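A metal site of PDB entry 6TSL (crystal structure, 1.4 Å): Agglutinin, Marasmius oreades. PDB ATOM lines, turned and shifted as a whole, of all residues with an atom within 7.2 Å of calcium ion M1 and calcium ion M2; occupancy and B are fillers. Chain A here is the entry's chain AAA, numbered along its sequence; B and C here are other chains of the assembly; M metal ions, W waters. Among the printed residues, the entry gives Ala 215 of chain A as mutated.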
ATOM      1  N   ARG A 209     -10.406  17.676  -7.318  1.00  0.00           N
ATOM      2  CA  ARG A 209     -11.815  17.340  -7.632  1.00  0.00           C
ATOM      3  C   ARG A 209     -11.886  16.777  -9.052  1.00  0.00           C
ATOM      4  O   ARG A 209     -11.302  17.407  -9.968  1.00  0.00           O
ATOM      5  CB  ARG A 209     -12.685  18.577  -7.503  1.00  0.00           C
ATOM      6  CG  ARG A 209     -12.737  19.139  -6.086  1.00  0.00           C
ATOM      7  CD  ARG A 209     -13.419  20.504  -6.021  1.00  0.00           C
ATOM      8  NE  ARG A 209     -14.773  20.439  -6.525  1.00  0.00           N
ATOM      9  CZ  ARG A 209     -15.529  21.485  -6.815  1.00  0.00           C
ATOM     10  NH1 ARG A 209     -15.095  22.709  -6.606  1.00  0.00           N
ATOM     11  NH2 ARG A 209     -16.733  21.299  -7.340  1.00  0.00           N
ATOM     12  N   GLU A 210     -12.641  15.699  -9.242  1.00  0.00           N
ATOM     13  CA  GLU A 210     -12.719  14.943 -10.518  1.00  0.00           C
ATOM     14  C   GLU A 210     -13.104  15.907 -11.644  1.00  0.00           C
ATOM     15  O   GLU A 210     -14.197  16.539 -11.525  1.00  0.00           O
ATOM     16  CB  GLU A 210     -13.723  13.798 -10.366  1.00  0.00           C
ATOM     17  CG  GLU A 210     -13.985  13.013 -11.630  1.00  0.00           C
ATOM     18  CD  GLU A 210     -15.121  11.995 -11.497  1.00  0.00           C
ATOM     19  OE1 GLU A 210     -15.722  11.646 -12.517  1.00  0.00           O
ATOM     20  OE2 GLU A 210     -15.431  11.597 -10.363  1.00  0.00           O
ATOM     21  N   GLN A 211     -12.184  16.115 -12.614  1.00  0.00           N
ATOM     22  CA  GLN A 211     -12.337  16.932 -13.871  1.00  0.00           C
ATOM     23  C   GLN A 211     -12.355  18.449 -13.543  1.00  0.00           C
ATOM     24  O   GLN A 211     -11.726  19.213 -14.297  1.00  0.00           O
ATOM     25  CB  GLN A 211     -13.584  16.498 -14.665  1.00  0.00           C
ATOM     26  CG  GLN A 211     -13.434  15.100 -15.273  1.00  0.00           C
ATOM     27  CD  GLN A 211     -14.353  14.882 -16.463  1.00  0.00           C
ATOM     28  OE1 GLN A 211     -14.397  15.689 -17.402  1.00  0.00           O
ATOM     29  NE2 GLN A 211     -15.093  13.797 -16.427  1.00  0.00           N
ATOM     30  N   ILE A 212     -13.136  18.887 -12.544  1.00  0.00           N
ATOM     31  CA  ILE A 212     -13.453  20.328 -12.355  1.00  0.00           C
ATOM     32  C   ILE A 212     -12.225  21.051 -11.713  1.00  0.00           C
ATOM     33  O   ILE A 212     -12.053  22.259 -11.963  1.00  0.00           O
ATOM     34  CB  ILE A 212     -14.746  20.513 -11.521  1.00  0.00           C
ATOM     35  CG1 ILE A 212     -15.245  21.972 -11.562  1.00  0.00           C
ATOM     36  CG2 ILE A 212     -14.560  20.030 -10.111  1.00  0.00           C
ATOM     37  CD1 ILE A 212     -15.689  22.444 -12.922  1.00  0.00           C
ATOM     38  N   TYR A 213     -11.400  20.345 -10.965  1.00  0.00           N
ATOM     39  CA  TYR A 213     -10.077  20.908 -10.533  1.00  0.00           C
ATOM     40  C   TYR A 213      -9.115  19.773 -10.257  1.00  0.00           C
ATOM     41  O   TYR A 213      -8.883  19.433  -9.082  1.00  0.00           O
ATOM     42  CB  TYR A 213     -10.254  21.820  -9.304  1.00  0.00           C
ATOM     43  CG  TYR A 213      -9.330  23.012  -9.321  1.00  0.00           C
ATOM     44  CD1 TYR A 213      -9.551  24.055 -10.210  1.00  0.00           C
ATOM     45  CD2 TYR A 213      -8.144  23.014  -8.611  1.00  0.00           C
ATOM     46  CE1 TYR A 213      -8.696  25.129 -10.291  1.00  0.00           C
ATOM     47  CE2 TYR A 213      -7.230  24.038  -8.736  1.00  0.00           C
ATOM     48  CZ  TYR A 213      -7.526  25.126  -9.554  1.00  0.00           C
ATOM     49  OH  TYR A 213      -6.638  26.173  -9.668  1.00  0.00           O
ATOM     50  N   ASP A 214      -8.672  19.137 -11.308  1.00  0.00           N
ATOM     51  CA  ASP A 214      -7.798  17.963 -11.219  1.00  0.00           C
ATOM     52  C   ASP A 214      -6.396  18.379 -11.702  1.00  0.00           C
ATOM     53  O   ASP A 214      -6.104  19.576 -11.683  1.00  0.00           O
ATOM     54  CB  ASP A 214      -8.419  16.759 -11.971  1.00  0.00           C
ATOM     55  CG  ASP A 214      -8.530  16.939 -13.480  1.00  0.00           C
ATOM     56  OD1 ASP A 214      -8.725  18.061 -13.927  1.00  0.00           O
ATOM     57  OD2 ASP A 214      -8.550  15.877 -14.199  1.00  0.00           O
ATOM     58  N   ALA A 215      -5.544  17.421 -12.029  1.00  0.00           N
ATOM     59  CA  ALA A 215      -4.084  17.709 -12.196  1.00  0.00           C
ATOM     60  C   ALA A 215      -3.884  18.837 -13.232  1.00  0.00           C
ATOM     61  O   ALA A 215      -3.003  19.692 -13.013  1.00  0.00           O
ATOM     62  CB  ALA A 215      -3.339  16.438 -12.586  1.00  0.00           C
ATOM     63  N   ASP A 216      -4.611  18.796 -14.351  1.00  0.00           N
ATOM     64  CA  ASP A 216      -4.392  19.773 -15.444  1.00  0.00           C
ATOM     65  C   ASP A 216      -4.733  21.200 -14.942  1.00  0.00           C
ATOM     66  O   ASP A 216      -4.020  22.139 -15.312  1.00  0.00           O
ATOM     67  CB  ASP A 216      -5.174  19.392 -16.706  1.00  0.00           C
ATOM     68  CG  ASP A 216      -6.579  18.913 -16.441  1.00  0.00           C
ATOM     69  OD1 ASP A 216      -7.483  19.765 -16.369  1.00  0.00           O
ATOM     70  OD2 ASP A 216      -6.743  17.671 -16.201  1.00  0.00           O
ATOM     71  N   ASP A 217      -5.686  21.323 -14.042  1.00  0.00           N
ATOM     72  CA  ASP A 217      -6.065  22.659 -13.478  1.00  0.00           C
ATOM     73  C   ASP A 217      -4.919  23.165 -12.566  1.00  0.00           C
ATOM     74  O   ASP A 217      -4.583  24.371 -12.660  1.00  0.00           O
ATOM     75  CB  ASP A 217      -7.383  22.595 -12.758  1.00  0.00           C
ATOM     76  CG  ASP A 217      -8.535  22.196 -13.681  1.00  0.00           C
ATOM     77  OD1 ASP A 217      -8.924  23.042 -14.495  1.00  0.00           O
ATOM     78  OD2 ASP A 217      -8.850  21.026 -13.716  1.00  0.00           O
ATOM     79  N   PHE A 218      -4.350  22.296 -11.748  1.00  0.00           N
ATOM     80  CA  PHE A 218      -3.223  22.676 -10.832  1.00  0.00           C
ATOM     81  C   PHE A 218      -2.021  23.131 -11.676  1.00  0.00           C
ATOM     82  O   PHE A 218      -1.429  24.162 -11.371  1.00  0.00           O
ATOM     83  CB  PHE A 218      -2.853  21.523  -9.919  1.00  0.00           C
ATOM     84  CG  PHE A 218      -3.745  21.354  -8.728  1.00  0.00           C
ATOM     85  CD1 PHE A 218      -4.921  20.606  -8.819  1.00  0.00           C
ATOM     86  CD2 PHE A 218      -3.397  21.877  -7.499  1.00  0.00           C
ATOM     87  CE1 PHE A 218      -5.707  20.383  -7.693  1.00  0.00           C
ATOM     88  CE2 PHE A 218      -4.194  21.682  -6.387  1.00  0.00           C
ATOM     89  CZ  PHE A 218      -5.349  20.946  -6.493  1.00  0.00           C
ATOM     90  N   ALA A 258      -0.820  15.538 -15.052  1.00  0.00           N
ATOM     91  CA  ALA A 258      -0.292  16.863 -15.458  1.00  0.00           C
ATOM     92  C   ALA A 258       0.503  17.470 -14.298  1.00  0.00           C
ATOM     93  O   ALA A 258       0.127  17.229 -13.130  1.00  0.00           O
ATOM     94  CB  ALA A 258      -1.421  17.758 -15.867  1.00  0.00           C
ATOM     95  N   ILE B 181      -6.187  16.706 -25.199  1.00  0.00           N
ATOM     96  CA  ILE B 181      -7.453  16.690 -24.419  1.00  0.00           C
ATOM     97  C   ILE B 181      -7.109  16.515 -22.936  1.00  0.00           C
ATOM     98  O   ILE B 181      -6.289  15.675 -22.632  1.00  0.00           O
ATOM     99  CB  ILE B 181      -8.370  15.585 -24.942  1.00  0.00           C
ATOM    100  CG1 ILE B 181      -8.801  15.856 -26.387  1.00  0.00           C
ATOM    101  CG2 ILE B 181      -9.573  15.390 -24.017  1.00  0.00           C
ATOM    102  CD1 ILE B 181      -9.489  14.663 -27.078  1.00  0.00           C
ATOM    103  N   LEU B 182      -7.790  17.241 -22.059  1.00  0.00           N
ATOM    104  CA  LEU B 182      -7.415  17.306 -20.630  1.00  0.00           C
ATOM    105  C   LEU B 182      -8.499  16.633 -19.766  1.00  0.00           C
ATOM    106  O   LEU B 182      -8.182  16.227 -18.640  1.00  0.00           O
ATOM    107  CB  LEU B 182      -7.220  18.765 -20.230  1.00  0.00           C
ATOM    108  CG  LEU B 182      -6.093  19.508 -20.961  1.00  0.00           C
ATOM    109  CD1 LEU B 182      -6.044  20.979 -20.517  1.00  0.00           C
ATOM    110  CD2 LEU B 182      -4.757  18.847 -20.739  1.00  0.00           C
ATOM    111  N   ASP B 183      -9.769  16.675 -20.220  1.00  0.00           N
ATOM    112  CA  ASP B 183     -10.929  16.202 -19.413  1.00  0.00           C
ATOM    113  C   ASP B 183     -11.918  15.466 -20.335  1.00  0.00           C
ATOM    114  O   ASP B 183     -11.521  15.146 -21.476  1.00  0.00           O
ATOM    115  CB  ASP B 183     -11.598  17.366 -18.665  1.00  0.00           C
ATOM    116  CG  ASP B 183     -10.678  18.080 -17.642  1.00  0.00           C
ATOM    117  OD1 ASP B 183     -10.227  17.424 -16.693  1.00  0.00           O
ATOM    118  OD2 ASP B 183     -10.516  19.321 -17.774  1.00  0.00           O
ATOM    119  N   GLY B 184     -13.078  15.116 -19.819  1.00  0.00           N
ATOM    120  CA  GLY B 184     -14.011  14.170 -20.494  1.00  0.00           C
ATOM    121  C   GLY B 184     -15.294  14.866 -20.941  1.00  0.00           C
ATOM    122  O   GLY B 184     -15.871  14.411 -21.932  1.00  0.00           O
ATOM    123  N   TYR B 186     -17.576  18.671 -20.752  1.00  0.00           N
ATOM    124  CA  TYR B 186     -17.364  20.129 -20.574  1.00  0.00           C
ATOM    125  C   TYR B 186     -18.713  20.859 -20.603  1.00  0.00           C
ATOM    126  O   TYR B 186     -19.386  20.845 -21.657  1.00  0.00           O
ATOM    127  CB  TYR B 186     -16.460  20.675 -21.655  1.00  0.00           C
ATOM    128  CG  TYR B 186     -15.101  20.053 -21.713  1.00  0.00           C
ATOM    129  CD1 TYR B 186     -14.872  18.905 -22.459  1.00  0.00           C
ATOM    130  CD2 TYR B 186     -14.023  20.640 -21.080  1.00  0.00           C
ATOM    131  CE1 TYR B 186     -13.593  18.392 -22.622  1.00  0.00           C
ATOM    132  CE2 TYR B 186     -12.753  20.123 -21.202  1.00  0.00           C
ATOM    133  CZ  TYR B 186     -12.530  18.982 -21.970  1.00  0.00           C
ATOM    134  OH  TYR B 186     -11.264  18.504 -22.153  1.00  0.00           O
ATOM    135  N   LYS B 223      -7.412  30.706 -19.519  1.00  0.00           N
ATOM    136  CA  LYS B 223      -7.749  29.303 -19.208  1.00  0.00           C
ATOM    137  C   LYS B 223      -7.731  29.089 -17.677  1.00  0.00           C
ATOM    138  O   LYS B 223      -8.636  28.429 -17.176  1.00  0.00           O
ATOM    139  CB  LYS B 223      -6.803  28.318 -19.896  1.00  0.00           C
ATOM    140  CG  LYS B 223      -7.150  26.855 -19.688  1.00  0.00           C
ATOM    141  CD  LYS B 223      -6.958  25.989 -20.923  1.00  0.00           C
ATOM    142  CE  LYS B 223      -7.218  24.504 -20.665  1.00  0.00           C
ATOM    143  NZ  LYS B 223      -8.455  24.290 -19.858  1.00  0.00           N
ATOM    144  N   PHE B 239     -17.084  16.953 -14.167  1.00  0.00           N
ATOM    145  CA  PHE B 239     -17.141  17.729 -15.409  1.00  0.00           C
ATOM    146  C   PHE B 239     -16.098  18.858 -15.345  1.00  0.00           C
ATOM    147  O   PHE B 239     -15.636  19.201 -14.208  1.00  0.00           O
ATOM    148  CB  PHE B 239     -18.546  18.305 -15.626  1.00  0.00           C
ATOM    149  CG  PHE B 239     -18.917  19.371 -14.635  1.00  0.00           C
ATOM    150  CD1 PHE B 239     -19.185  19.054 -13.325  1.00  0.00           C
ATOM    151  CD2 PHE B 239     -18.859  20.709 -14.994  1.00  0.00           C
ATOM    152  CE1 PHE B 239     -19.419  20.049 -12.387  1.00  0.00           C
ATOM    153  CE2 PHE B 239     -19.141  21.697 -14.067  1.00  0.00           C
ATOM    154  CZ  PHE B 239     -19.403  21.375 -12.777  1.00  0.00           C
ATOM    155  N   ALA B 240     -15.844  19.498 -16.470  1.00  0.00           N
ATOM    156  CA  ALA B 240     -14.983  20.683 -16.572  1.00  0.00           C
ATOM    157  C   ALA B 240     -15.723  21.789 -17.324  1.00  0.00           C
ATOM    158  O   ALA B 240     -16.859  21.546 -17.777  1.00  0.00           O
ATOM    159  CB  ALA B 240     -13.679  20.309 -17.259  1.00  0.00           C
ATOM    160  N   ILE B 241     -15.163  22.982 -17.340  1.00  0.00           N
ATOM    161  CA  ILE B 241     -15.688  24.111 -18.141  1.00  0.00           C
ATOM    162  C   ILE B 241     -14.918  24.171 -19.448  1.00  0.00           C
ATOM    163  O   ILE B 241     -13.640  24.104 -19.401  1.00  0.00           O
ATOM    164  CB  ILE B 241     -15.572  25.440 -17.365  1.00  0.00           C
ATOM    165  CG1 ILE B 241     -16.031  25.312 -15.903  1.00  0.00           C
ATOM    166  CG2 ILE B 241     -16.326  26.540 -18.091  1.00  0.00           C
ATOM    167  CD1 ILE B 241     -17.420  24.757 -15.745  1.00  0.00           C
ATOM    168  N   TYR B 293      -7.248  21.657 -24.249  1.00  0.00           N
ATOM    169  CA  TYR B 293      -8.610  21.972 -23.777  1.00  0.00           C
ATOM    170  C   TYR B 293      -9.107  20.823 -22.939  1.00  0.00           C
ATOM    171  O   TYR B 293      -9.889  21.013 -22.019  1.00  0.00           O
ATOM    172  CB  TYR B 293      -9.545  22.241 -24.959  1.00  0.00           C
ATOM    173  CG  TYR B 293      -9.591  21.119 -25.987  1.00  0.00           C
ATOM    174  CD1 TYR B 293      -8.651  21.031 -27.002  1.00  0.00           C
ATOM    175  CD2 TYR B 293     -10.605  20.176 -25.952  1.00  0.00           C
ATOM    176  CE1 TYR B 293      -8.713  20.022 -27.955  1.00  0.00           C
ATOM    177  CE2 TYR B 293     -10.686  19.164 -26.909  1.00  0.00           C
ATOM    178  CZ  TYR B 293      -9.748  19.098 -27.930  1.00  0.00           C
ATOM    179  OH  TYR B 293      -9.832  18.092 -28.880  1.00  0.00           O
ATOM    180  OXT TYR B 293      -8.697  19.670 -23.171  1.00  0.00           O
ATOM    181  N   VAL C   2      -6.345  10.142 -20.285  1.00  0.00           N
ATOM    182  CA  VAL C   2      -6.561  11.599 -20.140  1.00  0.00           C
ATOM    183  C   VAL C   2      -6.030  12.031 -18.769  1.00  0.00           C
ATOM    184  O   VAL C   2      -6.203  11.323 -17.774  1.00  0.00           O
ATOM    185  CB  VAL C   2      -8.053  11.966 -20.310  1.00  0.00           C
ATOM    186  CG1 VAL C   2      -8.924  11.366 -19.200  1.00  0.00           C
ATOM    187  CG2 VAL C   2      -8.261  13.470 -20.390  1.00  0.00           C
ATOM    188  N   PRO C   3      -5.306  13.176 -18.685  1.00  0.00           N
ATOM    189  CA  PRO C   3      -4.602  13.550 -17.446  1.00  0.00           C
ATOM    190  C   PRO C   3      -5.570  13.788 -16.282  1.00  0.00           C
ATOM    191  O   PRO C   3      -6.584  14.473 -16.475  1.00  0.00           O
ATOM    192  CB  PRO C   3      -3.823  14.862 -17.804  1.00  0.00           C
ATOM    193  CG  PRO C   3      -4.380  15.292 -19.184  1.00  0.00           C
ATOM    194  CD  PRO C   3      -4.935  14.034 -19.813  1.00  0.00           C
ATOM    195  N   ARG C   4      -5.241  13.238 -15.142  1.00  0.00           N
ATOM    196  CA  ARG C   4      -6.054  13.391 -13.906  1.00  0.00           C
ATOM    197  C   ARG C   4      -5.113  13.621 -12.732  1.00  0.00           C
ATOM    198  O   ARG C   4      -5.539  14.241 -11.701  1.00  0.00           O
ATOM    199  CB  ARG C   4      -6.925  12.150 -13.667  1.00  0.00           C
ATOM    200  CG  ARG C   4      -7.964  11.901 -14.754  1.00  0.00           C
ATOM    201  CD  ARG C   4      -8.679  10.565 -14.582  1.00  0.00           C
ATOM    202  NE  ARG C   4      -9.381  10.448 -13.297  1.00  0.00           N
ATOM    203  CZ  ARG C   4      -8.923   9.776 -12.225  1.00  0.00           C
ATOM    204  NH1 ARG C   4      -7.754   9.161 -12.277  1.00  0.00           N
ATOM    205  NH2 ARG C   4      -9.643   9.734 -11.117  1.00  0.00           N
ATOM    206  OXT ARG C   4      -3.900  13.194 -12.760  1.00  0.00           O
HETATM  207 CA    CA M   1      -9.689  19.577 -15.423  1.00  0.00          CA
HETATM  208 CA    CA M   2      -8.335  16.002 -16.448  1.00  0.00          CA
HETATM  209  O   HOH W   1      -9.873  14.023 -16.648  1.00  0.00           O
HETATM  210  O   HOH W   2     -10.452  21.735 -16.110  1.00  0.00           O
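Along chain A the residues within 4 Å of calcium ion M2 span positions 214 to 216.
The nearest printed residue that does not touch calcium ion M2 is Arg 4 of chain C (4.3 Å).
The backbone NH (N) of Asp 183 of chain B is in hydrogen-bond range of the side-chain hydroxyl (OH) of Tyr 186 of chain B, 3.1 Å away.
The backbone NH (N) of Gly 184 of chain B is in hydrogen-bond range of the side-chain amide oxygen (OE1) of Gln 211.
The backbone carbonyl oxygen (O) of Arg 209 is in hydrogen-bond range of the backbone NH (N) of Asp 214 (3.4 Å).
The chain-end carboxylate (OXT) of Tyr 293 of chain B is in hydrogen-bond range of the backbone NH (N) of Leu 182 of chain B, 2.8 Å away.
Within 4 Å of calcium ion M1: Gln 211, Asp 214, Asp 216, Asp 217 and Asp 183 of chain B.
Along chain A the residues within 4 Å of calcium ion M1 span positions 211 to 217.
The nearest printed residue that does not touch calcium ion M1 is Ala 240 of chain B (4.5 Å).
Calcium ion M2 is bound by the backbone carbonyl oxygen (O) of Leu 182 of chain B (2.2 Å), the side-chain carboxylate (OD2) of Asp 214 (2.3 Å), the side-chain carboxylate (OD2) of Asp 216 (2.3 Å), the backbone carbonyl oxygen (O) of Pro 3 of chain C (2.3 Å), the side-chain carboxylate (OD1) of Asp 183 of chain B (2.4 Å) and water W1 (2.5 Å).
The side-chain carboxylate (OD1) of Asp 214 is bound to calcium ion M1, at 2.3 Å.
O of Gln 211 is bound to calcium ion M1, at 2.4 Å.
Water W2 binds calcium ion M1, at 2.4 Å.
The side-chain carboxylate (OD2) of Asp 217 is bound to calcium ion M1 (2.4 Å).
Calcium ion M1 is bound by OD1 of Asp 216, 2.4 Å away.
Calcium ion M1 is bound by OD2 of Asp 183 of chain B (2.5 Å).
Calcium ion M1 is bound by OD1 of Asp 183 of chain B (2.6 Å).
Calcium ion M1 has seven donor atoms within binding distance.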
